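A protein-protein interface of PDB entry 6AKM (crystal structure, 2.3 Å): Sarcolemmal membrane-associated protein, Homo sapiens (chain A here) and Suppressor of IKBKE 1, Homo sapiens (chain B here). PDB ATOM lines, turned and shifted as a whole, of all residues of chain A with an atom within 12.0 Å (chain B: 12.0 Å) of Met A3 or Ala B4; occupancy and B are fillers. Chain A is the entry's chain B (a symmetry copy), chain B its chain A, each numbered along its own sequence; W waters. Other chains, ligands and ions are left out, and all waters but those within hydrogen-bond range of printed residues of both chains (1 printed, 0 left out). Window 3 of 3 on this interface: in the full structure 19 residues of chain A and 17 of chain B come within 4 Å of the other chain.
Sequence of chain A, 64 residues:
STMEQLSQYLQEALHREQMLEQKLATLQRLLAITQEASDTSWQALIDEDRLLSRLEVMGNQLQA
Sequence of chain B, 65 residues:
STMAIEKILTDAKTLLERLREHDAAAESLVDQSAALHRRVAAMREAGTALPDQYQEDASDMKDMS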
ATOM      1  N   SER A   1      -9.072  -5.679   0.376  1.00  0.00           N
ATOM      2  CA  SER A   1      -8.449  -6.623  -0.541  1.00  0.00           C
ATOM      3  C   SER A   1      -7.361  -5.937  -1.346  1.00  0.00           C
ATOM      4  O   SER A   1      -7.602  -4.911  -1.984  1.00  0.00           O
ATOM      5  CB  SER A   1      -9.490  -7.235  -1.478  1.00  0.00           C
ATOM      6  OG  SER A   1      -8.897  -8.177  -2.353  1.00  0.00           O
ATOM      7  N   THR A   2      -6.154  -6.503  -1.324  1.00  0.00           N
ATOM      8  CA  THR A   2      -5.067  -5.891  -2.077  1.00  0.00           C
ATOM      9  C   THR A   2      -5.215  -6.116  -3.580  1.00  0.00           C
ATOM     10  O   THR A   2      -4.755  -5.291  -4.373  1.00  0.00           O
ATOM     11  CB  THR A   2      -3.720  -6.414  -1.585  1.00  0.00           C
ATOM     12  OG1 THR A   2      -3.610  -7.804  -1.885  1.00  0.00           O
ATOM     13  CG2 THR A   2      -3.573  -6.200  -0.084  1.00  0.00           C
ATOM     14  N   MET A   3      -5.858  -7.205  -3.998  1.00  0.00           N
ATOM     15  CA  MET A   3      -6.003  -7.459  -5.426  1.00  0.00           C
ATOM     16  C   MET A   3      -7.200  -6.749  -6.048  1.00  0.00           C
ATOM     17  O   MET A   3      -7.366  -6.797  -7.274  1.00  0.00           O
ATOM     18  CB  MET A   3      -6.085  -8.960  -5.674  1.00  0.00           C
ATOM     19  CG  MET A   3      -4.969  -9.699  -4.969  1.00  0.00           C
ATOM     20  SD  MET A   3      -3.543  -9.763  -6.071  1.00  0.00           S
ATOM     21  CE  MET A   3      -4.282 -10.447  -7.544  1.00  0.00           C
ATOM     22  N   GLU A   4      -8.049  -6.132  -5.235  1.00  0.00           N
ATOM     23  CA  GLU A   4      -8.994  -5.150  -5.732  1.00  0.00           C
ATOM     24  C   GLU A   4      -8.421  -3.745  -5.692  1.00  0.00           C
ATOM     25  O   GLU A   4      -8.937  -2.869  -6.384  1.00  0.00           O
ATOM     26  CB  GLU A   4     -10.301  -5.192  -4.928  1.00  0.00           C
ATOM     27  N   GLN A   5      -7.368  -3.523  -4.905  1.00  0.00           N
ATOM     28  CA  GLN A   5      -6.752  -2.218  -4.729  1.00  0.00           C
ATOM     29  C   GLN A   5      -5.667  -1.980  -5.776  1.00  0.00           C
ATOM     30  O   GLN A   5      -5.585  -0.891  -6.365  1.00  0.00           O
ATOM     31  CB  GLN A   5      -6.200  -2.120  -3.306  1.00  0.00           C
ATOM     32  CG  GLN A   5      -4.953  -1.296  -3.141  1.00  0.00           C
ATOM     33  CD  GLN A   5      -4.724  -0.903  -1.694  1.00  0.00           C
ATOM     34  OE1 GLN A   5      -4.891  -1.718  -0.782  1.00  0.00           O
ATOM     35  NE2 GLN A   5      -4.362   0.360  -1.473  1.00  0.00           N
ATOM     36  N   LEU A   6      -4.842  -2.999  -6.009  1.00  0.00           N
ATOM     37  CA  LEU A   6      -4.086  -3.162  -7.241  1.00  0.00           C
ATOM     38  C   LEU A   6      -4.875  -2.760  -8.470  1.00  0.00           C
ATOM     39  O   LEU A   6      -4.576  -1.741  -9.107  1.00  0.00           O
ATOM     40  CB  LEU A   6      -3.676  -4.612  -7.406  1.00  0.00           C
ATOM     41  CG  LEU A   6      -2.433  -4.930  -8.214  1.00  0.00           C
ATOM     42  CD1 LEU A   6      -1.152  -4.548  -7.485  1.00  0.00           C
ATOM     43  CD2 LEU A   6      -2.461  -6.410  -8.469  1.00  0.00           C
ATOM     44  N   SER A   7      -5.870  -3.580  -8.816  1.00  0.00           N
ATOM     45  CA  SER A   7      -6.609  -3.419 -10.061  1.00  0.00           C
ATOM     46  C   SER A   7      -7.160  -2.002 -10.192  1.00  0.00           C
ATOM     47  O   SER A   7      -7.388  -1.527 -11.309  1.00  0.00           O
ATOM     48  CB  SER A   7      -7.736  -4.450 -10.160  1.00  0.00           C
ATOM     49  OG  SER A   7      -7.983  -4.783 -11.515  1.00  0.00           O
ATOM     50  N   GLN A   8      -7.348  -1.315  -9.059  1.00  0.00           N
ATOM     51  CA  GLN A   8      -7.724   0.095  -9.097  1.00  0.00           C
ATOM     52  C   GLN A   8      -6.528   0.977  -9.451  1.00  0.00           C
ATOM     53  O   GLN A   8      -6.617   1.811 -10.357  1.00  0.00           O
ATOM     54  CB  GLN A   8      -8.332   0.524  -7.761  1.00  0.00           C
ATOM     55  N   TYR A   9      -5.407   0.814  -8.736  1.00  0.00           N
ATOM     56  CA  TYR A   9      -4.196   1.586  -9.013  1.00  0.00           C
ATOM     57  C   TYR A   9      -3.806   1.488 -10.481  1.00  0.00           C
ATOM     58  O   TYR A   9      -3.534   2.501 -11.139  1.00  0.00           O
ATOM     59  CB  TYR A   9      -3.042   1.083  -8.147  1.00  0.00           C
ATOM     60  CG  TYR A   9      -3.036   1.554  -6.714  1.00  0.00           C
ATOM     61  CD1 TYR A   9      -3.840   2.607  -6.292  1.00  0.00           C
ATOM     62  CD2 TYR A   9      -2.194   0.950  -5.779  1.00  0.00           C
ATOM     63  CE1 TYR A   9      -3.827   3.026  -4.963  1.00  0.00           C
ATOM     64  CE2 TYR A   9      -2.175   1.350  -4.457  1.00  0.00           C
ATOM     65  CZ  TYR A   9      -2.989   2.392  -4.055  1.00  0.00           C
ATOM     66  OH  TYR A   9      -2.958   2.794  -2.739  1.00  0.00           O
ATOM     67  N   LEU A  10      -3.772   0.264 -11.009  1.00  0.00           N
ATOM     68  CA  LEU A  10      -3.366   0.066 -12.394  1.00  0.00           C
ATOM     69  C   LEU A  10      -4.358   0.704 -13.355  1.00  0.00           C
ATOM     70  O   LEU A  10      -3.966   1.445 -14.264  1.00  0.00           O
ATOM     71  CB  LEU A  10      -3.214  -1.420 -12.697  1.00  0.00           C
ATOM     72  CG  LEU A  10      -1.774  -1.926 -12.678  1.00  0.00           C
ATOM     73  CD1 LEU A  10      -1.178  -1.819 -11.273  1.00  0.00           C
ATOM     74  CD2 LEU A  10      -1.701  -3.351 -13.209  1.00  0.00           C
ATOM     75  N   GLN A  11      -5.649   0.419 -13.174  1.00  0.00           N
ATOM     76  CA  GLN A  11      -6.650   0.996 -14.063  1.00  0.00           C
ATOM     77  C   GLN A  11      -6.640   2.523 -14.011  1.00  0.00           C
ATOM     78  O   GLN A  11      -6.931   3.182 -15.016  1.00  0.00           O
ATOM     79  CB  GLN A  11      -8.033   0.456 -13.710  1.00  0.00           C
ATOM     80  CG  GLN A  11      -8.362  -0.876 -14.372  1.00  0.00           C
ATOM     81  CD  GLN A  11      -8.926  -0.710 -15.777  1.00  0.00           C
ATOM     82  OE1 GLN A  11      -8.506  -1.403 -16.710  1.00  0.00           O
ATOM     83  NE2 GLN A  11      -9.875   0.219 -15.936  1.00  0.00           N
ATOM     84  N   GLU A  12      -6.315   3.100 -12.856  1.00  0.00           N
ATOM     85  CA  GLU A  12      -6.241   4.545 -12.746  1.00  0.00           C
ATOM     86  C   GLU A  12      -4.908   5.091 -13.243  1.00  0.00           C
ATOM     87  O   GLU A  12      -4.859   6.221 -13.743  1.00  0.00           O
ATOM     88  CB  GLU A  12      -6.506   4.981 -11.302  1.00  0.00           C
ATOM     89  CG  GLU A  12      -5.311   4.943 -10.378  1.00  0.00           C
ATOM     90  CD  GLU A  12      -5.614   5.554  -9.022  1.00  0.00           C
ATOM     91  N   LEU A  14      -3.463   3.682 -15.836  1.00  0.00           N
ATOM     92  CA  LEU A  14      -3.713   3.686 -17.273  1.00  0.00           C
ATOM     93  C   LEU A  14      -4.545   4.895 -17.680  1.00  0.00           C
ATOM     94  O   LEU A  14      -4.275   5.528 -18.708  1.00  0.00           O
ATOM     95  CB  LEU A  14      -4.391   2.389 -17.702  1.00  0.00           C
ATOM     96  CG  LEU A  14      -3.441   1.188 -17.745  1.00  0.00           C
ATOM     97  CD1 LEU A  14      -4.130  -0.088 -17.216  1.00  0.00           C
ATOM     98  CD2 LEU A  14      -2.874   0.976 -19.140  1.00  0.00           C
ATOM     99  N   THR B   2     -10.421 -16.464 -15.185  1.00  0.00           N
ATOM    100  CA  THR B   2     -11.281 -15.868 -14.170  1.00  0.00           C
ATOM    101  C   THR B   2     -10.454 -15.175 -13.093  1.00  0.00           C
ATOM    102  O   THR B   2     -10.918 -14.224 -12.457  1.00  0.00           O
ATOM    103  CB  THR B   2     -12.192 -16.923 -13.508  1.00  0.00           C
ATOM    104  N   MET B   3      -9.226 -15.651 -12.899  1.00  0.00           N
ATOM    105  CA  MET B   3      -8.384 -15.128 -11.834  1.00  0.00           C
ATOM    106  C   MET B   3      -8.015 -13.672 -12.102  1.00  0.00           C
ATOM    107  O   MET B   3      -8.054 -13.186 -13.236  1.00  0.00           O
ATOM    108  CB  MET B   3      -7.128 -15.982 -11.669  1.00  0.00           C
ATOM    109  CG  MET B   3      -7.404 -17.345 -11.036  1.00  0.00           C
ATOM    110  SD  MET B   3      -8.572 -17.228  -9.658  1.00  0.00           S
ATOM    111  CE  MET B   3      -7.467 -17.043  -8.261  1.00  0.00           C
ATOM    112  N   ALA B   4      -7.595 -13.043 -11.032  1.00  0.00           N
ATOM    113  CA  ALA B   4      -7.344 -11.597 -11.020  1.00  0.00           C
ATOM    114  C   ALA B   4      -6.177 -11.208 -11.911  1.00  0.00           C
ATOM    115  O   ALA B   4      -6.388 -10.388 -12.809  1.00  0.00           O
ATOM    116  CB  ALA B   4      -7.141 -11.112  -9.613  1.00  0.00           C
ATOM    117  N   ILE B   5      -5.012 -11.712 -11.617  1.00  0.00           N
ATOM    118  CA  ILE B   5      -3.776 -11.316 -12.336  1.00  0.00           C
ATOM    119  C   ILE B   5      -3.958 -11.387 -13.844  1.00  0.00           C
ATOM    120  O   ILE B   5      -3.345 -10.612 -14.486  1.00  0.00           O
ATOM    121  CB  ILE B   5      -2.646 -12.199 -11.841  1.00  0.00           C
ATOM    122  CG1 ILE B   5      -2.941 -13.663 -12.164  1.00  0.00           C
ATOM    123  CG2 ILE B   5      -2.491 -11.958 -10.352  1.00  0.00           C
ATOM    124  CD1 ILE B   5      -2.245 -14.223 -13.376  1.00  0.00           C
ATOM    125  N   GLU B   6      -4.776 -12.254 -14.383  1.00  0.00           N
ATOM    126  CA  GLU B   6      -4.897 -12.288 -15.838  1.00  0.00           C
ATOM    127  C   GLU B   6      -5.213 -10.902 -16.405  1.00  0.00           C
ATOM    128  O   GLU B   6      -4.673 -10.514 -17.447  1.00  0.00           O
ATOM    129  CB  GLU B   6      -5.966 -13.302 -16.254  1.00  0.00           C
ATOM    130  N   LYS B   7      -6.073 -10.137 -15.724  1.00  0.00           N
ATOM    131  CA  LYS B   7      -6.366  -8.766 -16.131  1.00  0.00           C
ATOM    132  C   LYS B   7      -5.361  -7.752 -15.591  1.00  0.00           C
ATOM    133  O   LYS B   7      -5.136  -6.721 -16.238  1.00  0.00           O
ATOM    134  CB  LYS B   7      -7.777  -8.360 -15.694  1.00  0.00           C
ATOM    135  N   ILE B   8      -4.763  -7.996 -14.423  1.00  0.00           N
ATOM    136  CA  ILE B   8      -3.682  -7.139 -13.941  1.00  0.00           C
ATOM    137  C   ILE B   8      -2.462  -7.230 -14.847  1.00  0.00           C
ATOM    138  O   ILE B   8      -1.989  -6.205 -15.355  1.00  0.00           O
ATOM    139  CB  ILE B   8      -3.315  -7.457 -12.480  1.00  0.00           C
ATOM    140  CG1 ILE B   8      -4.568  -7.437 -11.601  1.00  0.00           C
ATOM    141  CG2 ILE B   8      -2.154  -6.598 -11.986  1.00  0.00           C
ATOM    142  CD1 ILE B   8      -4.547  -8.481 -10.503  1.00  0.00           C
ATOM    143  N   LEU B   9      -1.943  -8.441 -15.065  1.00  0.00           N
ATOM    144  CA  LEU B   9      -0.754  -8.580 -15.902  1.00  0.00           C
ATOM    145  C   LEU B   9      -0.962  -7.939 -17.268  1.00  0.00           C
ATOM    146  O   LEU B   9      -0.056  -7.282 -17.793  1.00  0.00           O
ATOM    147  CB  LEU B   9      -0.359 -10.055 -16.057  1.00  0.00           C
ATOM    148  N   THR B  10      -2.152  -8.111 -17.858  1.00  0.00           N
ATOM    149  CA  THR B  10      -2.428  -7.464 -19.138  1.00  0.00           C
ATOM    150  C   THR B  10      -2.386  -5.952 -18.997  1.00  0.00           C
ATOM    151  O   THR B  10      -1.892  -5.251 -19.888  1.00  0.00           O
ATOM    152  CB  THR B  10      -3.787  -7.886 -19.686  1.00  0.00           C
ATOM    153  OG1 THR B  10      -4.776  -7.717 -18.666  1.00  0.00           O
ATOM    154  CG2 THR B  10      -3.759  -9.338 -20.139  1.00  0.00           C
ATOM    155  N   ASP B  11      -2.900  -5.433 -17.876  1.00  0.00           N
ATOM    156  CA  ASP B  11      -2.917  -3.992 -17.657  1.00  0.00           C
ATOM    157  C   ASP B  11      -1.509  -3.455 -17.436  1.00  0.00           C
ATOM    158  O   ASP B  11      -1.134  -2.426 -18.018  1.00  0.00           O
ATOM    159  CB  ASP B  11      -3.825  -3.648 -16.471  1.00  0.00           C
ATOM    160  CG  ASP B  11      -5.307  -3.683 -16.834  1.00  0.00           C
ATOM    161  OD1 ASP B  11      -5.625  -3.935 -18.014  1.00  0.00           O
ATOM    162  OD2 ASP B  11      -6.154  -3.454 -15.941  1.00  0.00           O
ATOM    163  N   ALA B  12      -0.710  -4.149 -16.617  1.00  0.00           N
ATOM    164  CA  ALA B  12       0.673  -3.728 -16.412  1.00  0.00           C
ATOM    165  C   ALA B  12       1.476  -3.819 -17.705  1.00  0.00           C
ATOM    166  O   ALA B  12       2.285  -2.932 -18.002  1.00  0.00           O
ATOM    167  CB  ALA B  12       1.329  -4.560 -15.313  1.00  0.00           C
ATOM    168  N   LYS B  13       1.270  -4.886 -18.488  1.00  0.00           N
ATOM    169  CA  LYS B  13       1.941  -4.983 -19.782  1.00  0.00           C
ATOM    170  C   LYS B  13       1.498  -3.862 -20.719  1.00  0.00           C
ATOM    171  O   LYS B  13       2.302  -3.343 -21.502  1.00  0.00           O
ATOM    172  CB  LYS B  13       1.683  -6.347 -20.420  1.00  0.00           C
HETATM  173  O   HOH W   1      -6.206  -3.468 -13.379  1.00  0.00           O
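The side-chain amide oxygen of Gln A11 lies close to the side-chain carboxylate of Asp B11, at 3.2 Å.
Water W1 bridges OD2 of Asp B11 and OG of Ser A7.
CE of Met A3 touches CB of Ala B4, 3.6 Å away.
Met A3 touches Ile B5.
CE of Met A3 touches CD1 of Ile B8, 3.6 Å away.
Leu A6 touches Ile B8 (CD2 to CG2, 3.5 Å).
CG2 of Ile B8 touches CD2 of Leu A10 (3.5 Å).
Leu A10 touches Asp B11 (CD2 to CB, 3.9 Å).
N of Ala B12 touches CD2 of Leu A10, 3.6 Å away.
CD1 of Leu A14 touches CB of Asp B11 (3.6 Å).
Ser A1 touches none of the printed residues of chain B.
No residue of chain B comes within 4 Å of Thr A2.
Glu A4 touches none of the printed residues of chain B.
Leu A6 touches one residue of chain B.
Of the printed residues of chain B, Leu A10 touches Ile B8 (3.5 Å), Asp B11 (3.9 Å) and Ala B12 (3.6 Å).
Of the printed residues of chain B, Gln A11 touches Asp B11.
Printed residues of chain B within 4 Å of Leu A14: Asp B11 (3.6 Å).
Thr B2 touches none of the printed residues of chain A.
No residue of chain A comes within 4 Å of Met B3.
Ala B4 touches one residue of chain A.
Of the printed residues of chain A, Ile B5 touches Met A3.
No residue of chain A comes within 4 Å of Glu B6.
No residue of chain A comes within 4 Å of Lys B7.
The nearest residue of chain B that does not touch Met A3 is Met B3 (6.7 Å).
The nearest residue of chain A that does not touch Ala B4 is Ser A7 (6.0 Å).
The nearest printed residue of chain A that does not touch Ala B12 is Leu A14 (5.3 Å).
Printed residues of chain B that touch a printed residue of chain A: Ala B4, Ile B5, Ile B8, Asp B11 and Ala B12.
Hydrophobic or aromatic side chains of chain B within 4 Å of the printed part of chain A: Ala B4, Ile B5, Ile B8 and Ala B12.
Hydrophobic or aromatic side chains of chain A within 4 Å of the printed part of chain B: Met A3, Leu A6, Leu A10 and Leu A14.
Among the printed residues, no Asp or Glu carboxylate lies within 4 Å of a Lys or Arg side-chain nitrogen of the other chain.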
